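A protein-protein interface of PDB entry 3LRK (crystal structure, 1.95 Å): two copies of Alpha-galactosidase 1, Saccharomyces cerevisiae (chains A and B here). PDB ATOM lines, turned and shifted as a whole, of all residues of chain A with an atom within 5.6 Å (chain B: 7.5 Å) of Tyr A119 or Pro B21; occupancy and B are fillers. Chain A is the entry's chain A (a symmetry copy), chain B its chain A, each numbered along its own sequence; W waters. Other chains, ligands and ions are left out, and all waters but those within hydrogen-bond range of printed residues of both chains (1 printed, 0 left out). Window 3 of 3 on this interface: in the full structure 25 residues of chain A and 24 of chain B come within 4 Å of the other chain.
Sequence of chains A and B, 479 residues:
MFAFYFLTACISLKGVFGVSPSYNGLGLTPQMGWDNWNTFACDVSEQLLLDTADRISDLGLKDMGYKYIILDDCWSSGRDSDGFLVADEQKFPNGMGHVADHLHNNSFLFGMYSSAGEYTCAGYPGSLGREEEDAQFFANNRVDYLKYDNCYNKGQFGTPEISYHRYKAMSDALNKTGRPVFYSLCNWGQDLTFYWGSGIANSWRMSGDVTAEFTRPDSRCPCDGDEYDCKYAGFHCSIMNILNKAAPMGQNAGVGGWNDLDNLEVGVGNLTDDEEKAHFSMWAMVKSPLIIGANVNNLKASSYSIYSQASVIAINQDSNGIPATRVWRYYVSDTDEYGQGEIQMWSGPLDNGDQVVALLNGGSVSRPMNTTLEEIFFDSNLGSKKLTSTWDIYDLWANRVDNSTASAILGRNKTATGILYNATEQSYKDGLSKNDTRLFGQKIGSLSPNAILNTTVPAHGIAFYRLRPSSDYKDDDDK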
ATOM      1  N   SER A 115      -3.188 -21.439 -30.639  1.00  0.00           N
ATOM      2  CA  SER A 115      -3.172 -22.605 -29.755  1.00  0.00           C
ATOM      3  C   SER A 115      -3.732 -22.211 -28.408  1.00  0.00           C
ATOM      4  O   SER A 115      -3.481 -21.105 -27.932  1.00  0.00           O
ATOM      5  CB  SER A 115      -1.741 -23.142 -29.582  1.00  0.00           C
ATOM      6  OG  SER A 115      -1.718 -24.336 -28.814  1.00  0.00           O
ATOM      7  N   GLY A 117      -2.758 -22.594 -25.652  1.00  0.00           N
ATOM      8  CA  GLY A 117      -1.576 -22.799 -24.828  1.00  0.00           C
ATOM      9  C   GLY A 117      -0.767 -21.532 -24.759  1.00  0.00           C
ATOM     10  O   GLY A 117      -1.140 -20.513 -25.341  1.00  0.00           O
ATOM     11  N   GLU A 118       0.342 -21.607 -24.036  1.00  0.00           N
ATOM     12  CA  GLU A 118       1.255 -20.498 -23.881  1.00  0.00           C
ATOM     13  C   GLU A 118       1.880 -20.138 -25.236  1.00  0.00           C
ATOM     14  O   GLU A 118       2.093 -18.964 -25.538  1.00  0.00           O
ATOM     15  CB  GLU A 118       2.342 -20.892 -22.876  1.00  0.00           C
ATOM     16  CG  GLU A 118       3.258 -19.745 -22.503  1.00  0.00           C
ATOM     17  CD  GLU A 118       4.340 -20.133 -21.519  1.00  0.00           C
ATOM     18  OE1 GLU A 118       5.193 -19.263 -21.244  1.00  0.00           O
ATOM     19  OE2 GLU A 118       4.332 -21.286 -21.021  1.00  0.00           O
ATOM     20  N   TYR A 119       2.178 -21.174 -26.021  1.00  0.00           N
ATOM     21  CA  TYR A 119       2.765 -21.048 -27.352  1.00  0.00           C
ATOM     22  C   TYR A 119       2.006 -21.922 -28.321  1.00  0.00           C
ATOM     23  O   TYR A 119       1.306 -22.850 -27.917  1.00  0.00           O
ATOM     24  CB  TYR A 119       4.226 -21.523 -27.355  1.00  0.00           C
ATOM     25  CG  TYR A 119       5.089 -20.860 -26.323  1.00  0.00           C
ATOM     26  CD1 TYR A 119       5.433 -21.528 -25.139  1.00  0.00           C
ATOM     27  CD2 TYR A 119       5.554 -19.553 -26.511  1.00  0.00           C
ATOM     28  CE1 TYR A 119       6.240 -20.922 -24.186  1.00  0.00           C
ATOM     29  CE2 TYR A 119       6.350 -18.935 -25.564  1.00  0.00           C
ATOM     30  CZ  TYR A 119       6.684 -19.620 -24.402  1.00  0.00           C
ATOM     31  OH  TYR A 119       7.464 -18.998 -23.472  1.00  0.00           O
ATOM     32  N   THR A 120       2.180 -21.637 -29.611  1.00  0.00           N
ATOM     33  CA  THR A 120       1.692 -22.504 -30.665  1.00  0.00           C
ATOM     34  C   THR A 120       2.637 -23.693 -30.774  1.00  0.00           C
ATOM     35  O   THR A 120       3.694 -23.720 -30.139  1.00  0.00           O
ATOM     36  CB  THR A 120       1.607 -21.765 -32.010  1.00  0.00           C
ATOM     37  OG1 THR A 120       2.927 -21.387 -32.433  1.00  0.00           O
ATOM     38  CG2 THR A 120       0.734 -20.513 -31.873  1.00  0.00           C
ATOM     39  N   CYS A 121       2.267 -24.669 -31.591  1.00  0.00           N
ATOM     40  CA  CYS A 121       3.108 -25.849 -31.766  1.00  0.00           C
ATOM     41  C   CYS A 121       4.514 -25.537 -32.311  1.00  0.00           C
ATOM     42  O   CYS A 121       5.478 -26.212 -31.952  1.00  0.00           O
ATOM     43  CB  CYS A 121       2.390 -26.888 -32.612  1.00  0.00           C
ATOM     44  SG  CYS A 121       0.885 -27.519 -31.833  1.00  0.00           S
ATOM     45  N   GLY A 123       6.000 -22.714 -31.622  1.00  0.00           N
ATOM     46  CA  GLY A 123       6.613 -21.856 -30.603  1.00  0.00           C
ATOM     47  C   GLY A 123       6.345 -20.373 -30.700  1.00  0.00           C
ATOM     48  O   GLY A 123       7.063 -19.572 -30.097  1.00  0.00           O
ATOM     49  N   TYR A 124       5.313 -20.002 -31.460  1.00  0.00           N
ATOM     50  CA  TYR A 124       4.857 -18.616 -31.562  1.00  0.00           C
ATOM     51  C   TYR A 124       3.864 -18.317 -30.435  1.00  0.00           C
ATOM     52  O   TYR A 124       3.454 -19.238 -29.740  1.00  0.00           O
ATOM     53  CB  TYR A 124       4.222 -18.395 -32.943  1.00  0.00           C
ATOM     54  CG  TYR A 124       5.247 -18.497 -34.042  1.00  0.00           C
ATOM     55  CD1 TYR A 124       5.753 -19.742 -34.442  1.00  0.00           C
ATOM     56  CD2 TYR A 124       5.746 -17.346 -34.656  1.00  0.00           C
ATOM     57  CE1 TYR A 124       6.714 -19.837 -35.443  1.00  0.00           C
ATOM     58  CE2 TYR A 124       6.714 -17.432 -35.657  1.00  0.00           C
ATOM     59  CZ  TYR A 124       7.180 -18.677 -36.046  1.00  0.00           C
ATOM     60  OH  TYR A 124       8.117 -18.765 -37.037  1.00  0.00           O
ATOM     61  N   PRO A 125       3.503 -17.028 -30.225  1.00  0.00           N
ATOM     62  CA  PRO A 125       2.577 -16.674 -29.142  1.00  0.00           C
ATOM     63  C   PRO A 125       1.255 -17.434 -29.181  1.00  0.00           C
ATOM     64  O   PRO A 125       0.571 -17.450 -30.205  1.00  0.00           O
ATOM     65  CB  PRO A 125       2.333 -15.176 -29.347  1.00  0.00           C
ATOM     66  CG  PRO A 125       3.498 -14.700 -30.149  1.00  0.00           C
ATOM     67  CD  PRO A 125       3.980 -15.839 -30.964  1.00  0.00           C
ATOM     68  N   GLY A 126       0.917 -18.054 -28.053  1.00  0.00           N
ATOM     69  CA  GLY A 126      -0.337 -18.786 -27.896  1.00  0.00           C
ATOM     70  C   GLY A 126      -1.380 -17.971 -27.153  1.00  0.00           C
ATOM     71  O   GLY A 126      -1.062 -16.942 -26.546  1.00  0.00           O
ATOM     72  N   CYS A 151      -1.069 -27.363 -28.234  1.00  0.00           N
ATOM     73  CA  CYS A 151       0.319 -27.326 -27.765  1.00  0.00           C
ATOM     74  C   CYS A 151       0.513 -26.393 -26.577  1.00  0.00           C
ATOM     75  O   CYS A 151      -0.120 -25.347 -26.506  1.00  0.00           O
ATOM     76  CB  CYS A 151       1.251 -26.917 -28.907  1.00  0.00           C
ATOM     77  SG  CYS A 151       1.504 -28.289 -30.035  1.00  0.00           S
ATOM     78  N   TYR A 152       1.398 -26.790 -25.651  1.00  0.00           N
ATOM     79  CA  TYR A 152       1.800 -25.964 -24.496  1.00  0.00           C
ATOM     80  C   TYR A 152       0.646 -25.481 -23.620  1.00  0.00           C
ATOM     81  O   TYR A 152       0.559 -24.300 -23.253  1.00  0.00           O
ATOM     82  CB  TYR A 152       2.719 -24.814 -24.965  1.00  0.00           C
ATOM     83  CG  TYR A 152       3.889 -25.387 -25.724  1.00  0.00           C
ATOM     84  CD1 TYR A 152       3.982 -25.248 -27.111  1.00  0.00           C
ATOM     85  CD2 TYR A 152       4.875 -26.125 -25.059  1.00  0.00           C
ATOM     86  CE1 TYR A 152       5.037 -25.816 -27.824  1.00  0.00           C
ATOM     87  CE2 TYR A 152       5.943 -26.700 -25.763  1.00  0.00           C
ATOM     88  CZ  TYR A 152       6.021 -26.523 -27.140  1.00  0.00           C
ATOM     89  OH  TYR A 152       7.052 -27.093 -27.847  1.00  0.00           O
ATOM     90  N   VAL B  19       7.991 -26.991 -30.481  1.00  0.00           N
ATOM     91  CA  VAL B  19       9.072 -26.037 -30.057  1.00  0.00           C
ATOM     92  C   VAL B  19       8.504 -24.915 -29.222  1.00  0.00           C
ATOM     93  O   VAL B  19       7.387 -24.452 -29.455  1.00  0.00           O
ATOM     94  CB  VAL B  19       9.815 -25.374 -31.247  1.00  0.00           C
ATOM     95  CG1 VAL B  19      11.305 -25.677 -31.188  1.00  0.00           C
ATOM     96  CG2 VAL B  19       9.197 -25.767 -32.577  1.00  0.00           C
ATOM     97  N   SER B  20       9.288 -24.497 -28.240  1.00  0.00           N
ATOM     98  CA  SER B  20       8.981 -23.376 -27.377  1.00  0.00           C
ATOM     99  C   SER B  20      10.340 -22.935 -26.841  1.00  0.00           C
ATOM    100  O   SER B  20      11.261 -23.754 -26.799  1.00  0.00           O
ATOM    101  CB  SER B  20       8.051 -23.812 -26.232  1.00  0.00           C
ATOM    102  OG  SER B  20       8.699 -24.659 -25.290  1.00  0.00           O
ATOM    103  N   PRO B  21      10.482 -21.651 -26.445  1.00  0.00           N
ATOM    104  CA  PRO B  21      11.747 -21.262 -25.826  1.00  0.00           C
ATOM    105  C   PRO B  21      11.942 -21.954 -24.479  1.00  0.00           C
ATOM    106  O   PRO B  21      10.959 -22.356 -23.846  1.00  0.00           O
ATOM    107  CB  PRO B  21      11.599 -19.749 -25.614  1.00  0.00           C
ATOM    108  CG  PRO B  21      10.125 -19.484 -25.630  1.00  0.00           C
ATOM    109  CD  PRO B  21       9.534 -20.524 -26.545  1.00  0.00           C
ATOM    110  N   SER B  22      13.198 -22.095 -24.059  1.00  0.00           N
ATOM    111  CA  SER B  22      13.495 -22.554 -22.707  1.00  0.00           C
ATOM    112  C   SER B  22      12.776 -21.638 -21.713  1.00  0.00           C
ATOM    113  O   SER B  22      12.862 -20.425 -21.828  1.00  0.00           O
ATOM    114  CB  SER B  22      15.003 -22.519 -22.459  1.00  0.00           C
ATOM    115  OG  SER B  22      15.274 -22.732 -21.085  1.00  0.00           O
ATOM    116  N   TYR B  23      12.062 -22.205 -20.741  1.00  0.00           N
ATOM    117  CA  TYR B  23      11.305 -21.371 -19.791  1.00  0.00           C
ATOM    118  C   TYR B  23      12.176 -20.408 -18.947  1.00  0.00           C
ATOM    119  O   TYR B  23      11.724 -19.343 -18.536  1.00  0.00           O
ATOM    120  CB  TYR B  23      10.388 -22.245 -18.906  1.00  0.00           C
ATOM    121  CG  TYR B  23      11.004 -22.664 -17.578  1.00  0.00           C
ATOM    122  CD1 TYR B  23      10.604 -22.055 -16.387  1.00  0.00           C
ATOM    123  CD2 TYR B  23      11.981 -23.660 -17.518  1.00  0.00           C
ATOM    124  CE1 TYR B  23      11.173 -22.427 -15.151  1.00  0.00           C
ATOM    125  CE2 TYR B  23      12.556 -24.041 -16.286  1.00  0.00           C
ATOM    126  CZ  TYR B  23      12.135 -23.420 -15.116  1.00  0.00           C
ATOM    127  OH  TYR B  23      12.699 -23.776 -13.912  1.00  0.00           O
ATOM    128  N   ASN B  24      13.429 -20.791 -18.695  1.00  0.00           N
ATOM    129  CA  ASN B  24      14.332 -20.004 -17.840  1.00  0.00           C
ATOM    130  C   ASN B  24      15.689 -19.707 -18.481  1.00  0.00           C
ATOM    131  O   ASN B  24      16.587 -19.182 -17.810  1.00  0.00           O
ATOM    132  CB  ASN B  24      14.561 -20.701 -16.483  1.00  0.00           C
ATOM    133  CG  ASN B  24      15.260 -22.039 -16.626  1.00  0.00           C
ATOM    134  OD1 ASN B  24      15.484 -22.516 -17.743  1.00  0.00           O
ATOM    135  ND2 ASN B  24      15.619 -22.656 -15.492  1.00  0.00           N
ATOM    136  N   GLY B  25      15.845 -20.091 -19.748  1.00  0.00           N
ATOM    137  CA  GLY B  25      17.094 -19.885 -20.487  1.00  0.00           C
ATOM    138  C   GLY B  25      18.135 -20.978 -20.317  1.00  0.00           C
ATOM    139  O   GLY B  25      19.150 -20.965 -20.999  1.00  0.00           O
ATOM    140  N   LEU B  26      17.888 -21.928 -19.412  1.00  0.00           N
ATOM    141  CA  LEU B  26      18.805 -23.053 -19.199  1.00  0.00           C
ATOM    142  C   LEU B  26      18.360 -24.316 -19.948  1.00  0.00           C
ATOM    143  O   LEU B  26      17.302 -24.335 -20.575  1.00  0.00           O
ATOM    144  CB  LEU B  26      18.977 -23.334 -17.698  1.00  0.00           C
ATOM    145  CG  LEU B  26      19.590 -22.211 -16.851  1.00  0.00           C
ATOM    146  CD1 LEU B  26      19.434 -22.488 -15.348  1.00  0.00           C
ATOM    147  CD2 LEU B  26      21.077 -21.989 -17.221  1.00  0.00           C
ATOM    148  N   LEU B  28      19.663 -25.637 -22.639  1.00  0.00           N
ATOM    149  CA  LEU B  28      19.704 -25.487 -24.100  1.00  0.00           C
ATOM    150  C   LEU B  28      20.173 -26.776 -24.770  1.00  0.00           C
ATOM    151  O   LEU B  28      19.839 -27.040 -25.920  1.00  0.00           O
ATOM    152  CB  LEU B  28      20.548 -24.275 -24.523  1.00  0.00           C
ATOM    153  CG  LEU B  28      20.094 -22.925 -23.950  1.00  0.00           C
ATOM    154  CD1 LEU B  28      20.931 -21.795 -24.561  1.00  0.00           C
ATOM    155  CD2 LEU B  28      18.568 -22.660 -24.158  1.00  0.00           C
ATOM    156  N   SER B 198       7.650 -28.684 -19.802  1.00  0.00           N
ATOM    157  CA  SER B 198       8.502 -27.686 -20.488  1.00  0.00           C
ATOM    158  C   SER B 198       8.339 -26.241 -20.013  1.00  0.00           C
ATOM    159  O   SER B 198       9.324 -25.486 -19.939  1.00  0.00           O
ATOM    160  CB  SER B 198       8.349 -27.778 -22.013  1.00  0.00           C
ATOM    161  OG  SER B 198       7.086 -27.295 -22.435  1.00  0.00           O
ATOM    162  N   GLY B 199       7.110 -25.858 -19.676  1.00  0.00           N
ATOM    163  CA  GLY B 199       6.815 -24.494 -19.253  1.00  0.00           C
ATOM    164  C   GLY B 199       7.260 -24.119 -17.854  1.00  0.00           C
ATOM    165  O   GLY B 199       7.234 -22.937 -17.485  1.00  0.00           O
ATOM    166  N   VAL B 255      14.957 -28.242 -27.089  1.00  0.00           N
ATOM    167  CA  VAL B 255      15.706 -27.163 -26.446  1.00  0.00           C
ATOM    168  C   VAL B 255      14.968 -26.603 -25.226  1.00  0.00           C
ATOM    169  O   VAL B 255      13.824 -26.143 -25.346  1.00  0.00           O
ATOM    170  CB  VAL B 255      16.063 -26.019 -27.460  1.00  0.00           C
ATOM    171  CG1 VAL B 255      16.647 -24.811 -26.742  1.00  0.00           C
ATOM    172  CG2 VAL B 255      17.045 -26.535 -28.496  1.00  0.00           C
ATOM    173  N   GLY B 256      15.616 -26.685 -24.059  1.00  0.00           N
ATOM    174  CA  GLY B 256      15.062 -26.138 -22.824  1.00  0.00           C
ATOM    175  C   GLY B 256      14.314 -27.102 -21.908  1.00  0.00           C
ATOM    176  O   GLY B 256      14.114 -26.800 -20.741  1.00  0.00           O
ATOM    177  N   GLY B 257      13.895 -28.251 -22.429  1.00  0.00           N
ATOM    178  CA  GLY B 257      13.062 -29.192 -21.661  1.00  0.00           C
ATOM    179  C   GLY B 257      13.190 -30.605 -22.203  1.00  0.00           C
ATOM    180  O   GLY B 257      12.724 -30.892 -23.298  1.00  0.00           O
HETATM  181  O   HOH W   1       5.034 -21.688 -18.636  1.00  0.00           O
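OH of Tyr A152 sits at hydrogen-bond distance from N of Ser B20 (3.4 Å). N of Val B19 is in hydrogen-bond range of O of Cys A121 (3.0 Å). O of Val B19 sits close to N of Gly A123, at 3.1 Å. The backbone NH (N) of Val B19 lies within hydrogen-bond range of the side-chain hydroxyl (OH) of Tyr A152 (2.8 Å).
The side-chain sulfur of Cys A151 is disulfide-bonded to the side-chain sulfur of Cys A121 (2.1 Å). O of Tyr A152 sits at hydrogen-bond distance from N of Glu A118 (2.8 Å). OG1 of Thr A120 sits at hydrogen-bond distance from N of Gly A123, 3.4 Å away. The side-chain hydroxyl (OG) of Ser A115 sits close to the backbone carbonyl oxygen (O) of Tyr A119 (3.5 Å). The side-chain hydroxyl of Thr A120 lies within hydrogen-bond range of the backbone NH of Tyr A124 (2.9 Å). The side-chain carboxylate (OE1) of Glu A118 sits at hydrogen-bond distance from the side-chain hydroxyl (OH) of Tyr A119 (3.2 Å).
Among the printed residues, merely in contact across the chains: Tyr A119 with Ser B20 (3.6 Å), Tyr A119 with Pro B21 (3.5 Å), Thr A120 with Val B19 (3.8 Å) and Tyr A152 with Ser B198 (3.6 Å).
Of chain A, only Tyr A119 comes within 4 Å of Pro B21. Of the printed residues of chain B, Tyr A152 touches Val B19, Ser B20 and Ser B198. Of the printed residues of chain A, Val B19 touches Thr A120, Cys A121, Gly A123 and Tyr A152. Tyr A124 touches none of the printed residues of chain B. Ser A115 touches none of the printed residues of chain B. The nearest residue of chain B that does not touch Tyr A119 is Val B19 (4.8 Å). The nearest residue of chain A that does not touch Pro B21 is Gly A123 (4.4 Å).
Of the 14 printed residues of chain B, 4 touch a printed residue of chain A. Hydrophobic or aromatic side chains of chain B that line the printed part of chain A: Val B19 and Pro B21. Printed residues of chain A that touch a printed residue of chain B: Tyr A119, Thr A120, Cys A121, Gly A123 and Tyr A152. Hydrophobic or aromatic side chains of chain A that line the printed part of chain B: Tyr A119 and Tyr A152. Among the printed residues, 8 pairs touch across the chains. Among the printed residues, no Asp or Glu carboxylate lies within 4 Å of a Lys or Arg side-chain nitrogen of the other chain.
No position is printed for both chains. Of the 8 pairs that touch across the chains among the printed residues, none has its exchanged pair printed and touching as well.
Water W1 lies within hydrogen-bond range of OE2 of Glu A118 (2.5 Å) and O of Gly B199 (2.8 Å).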
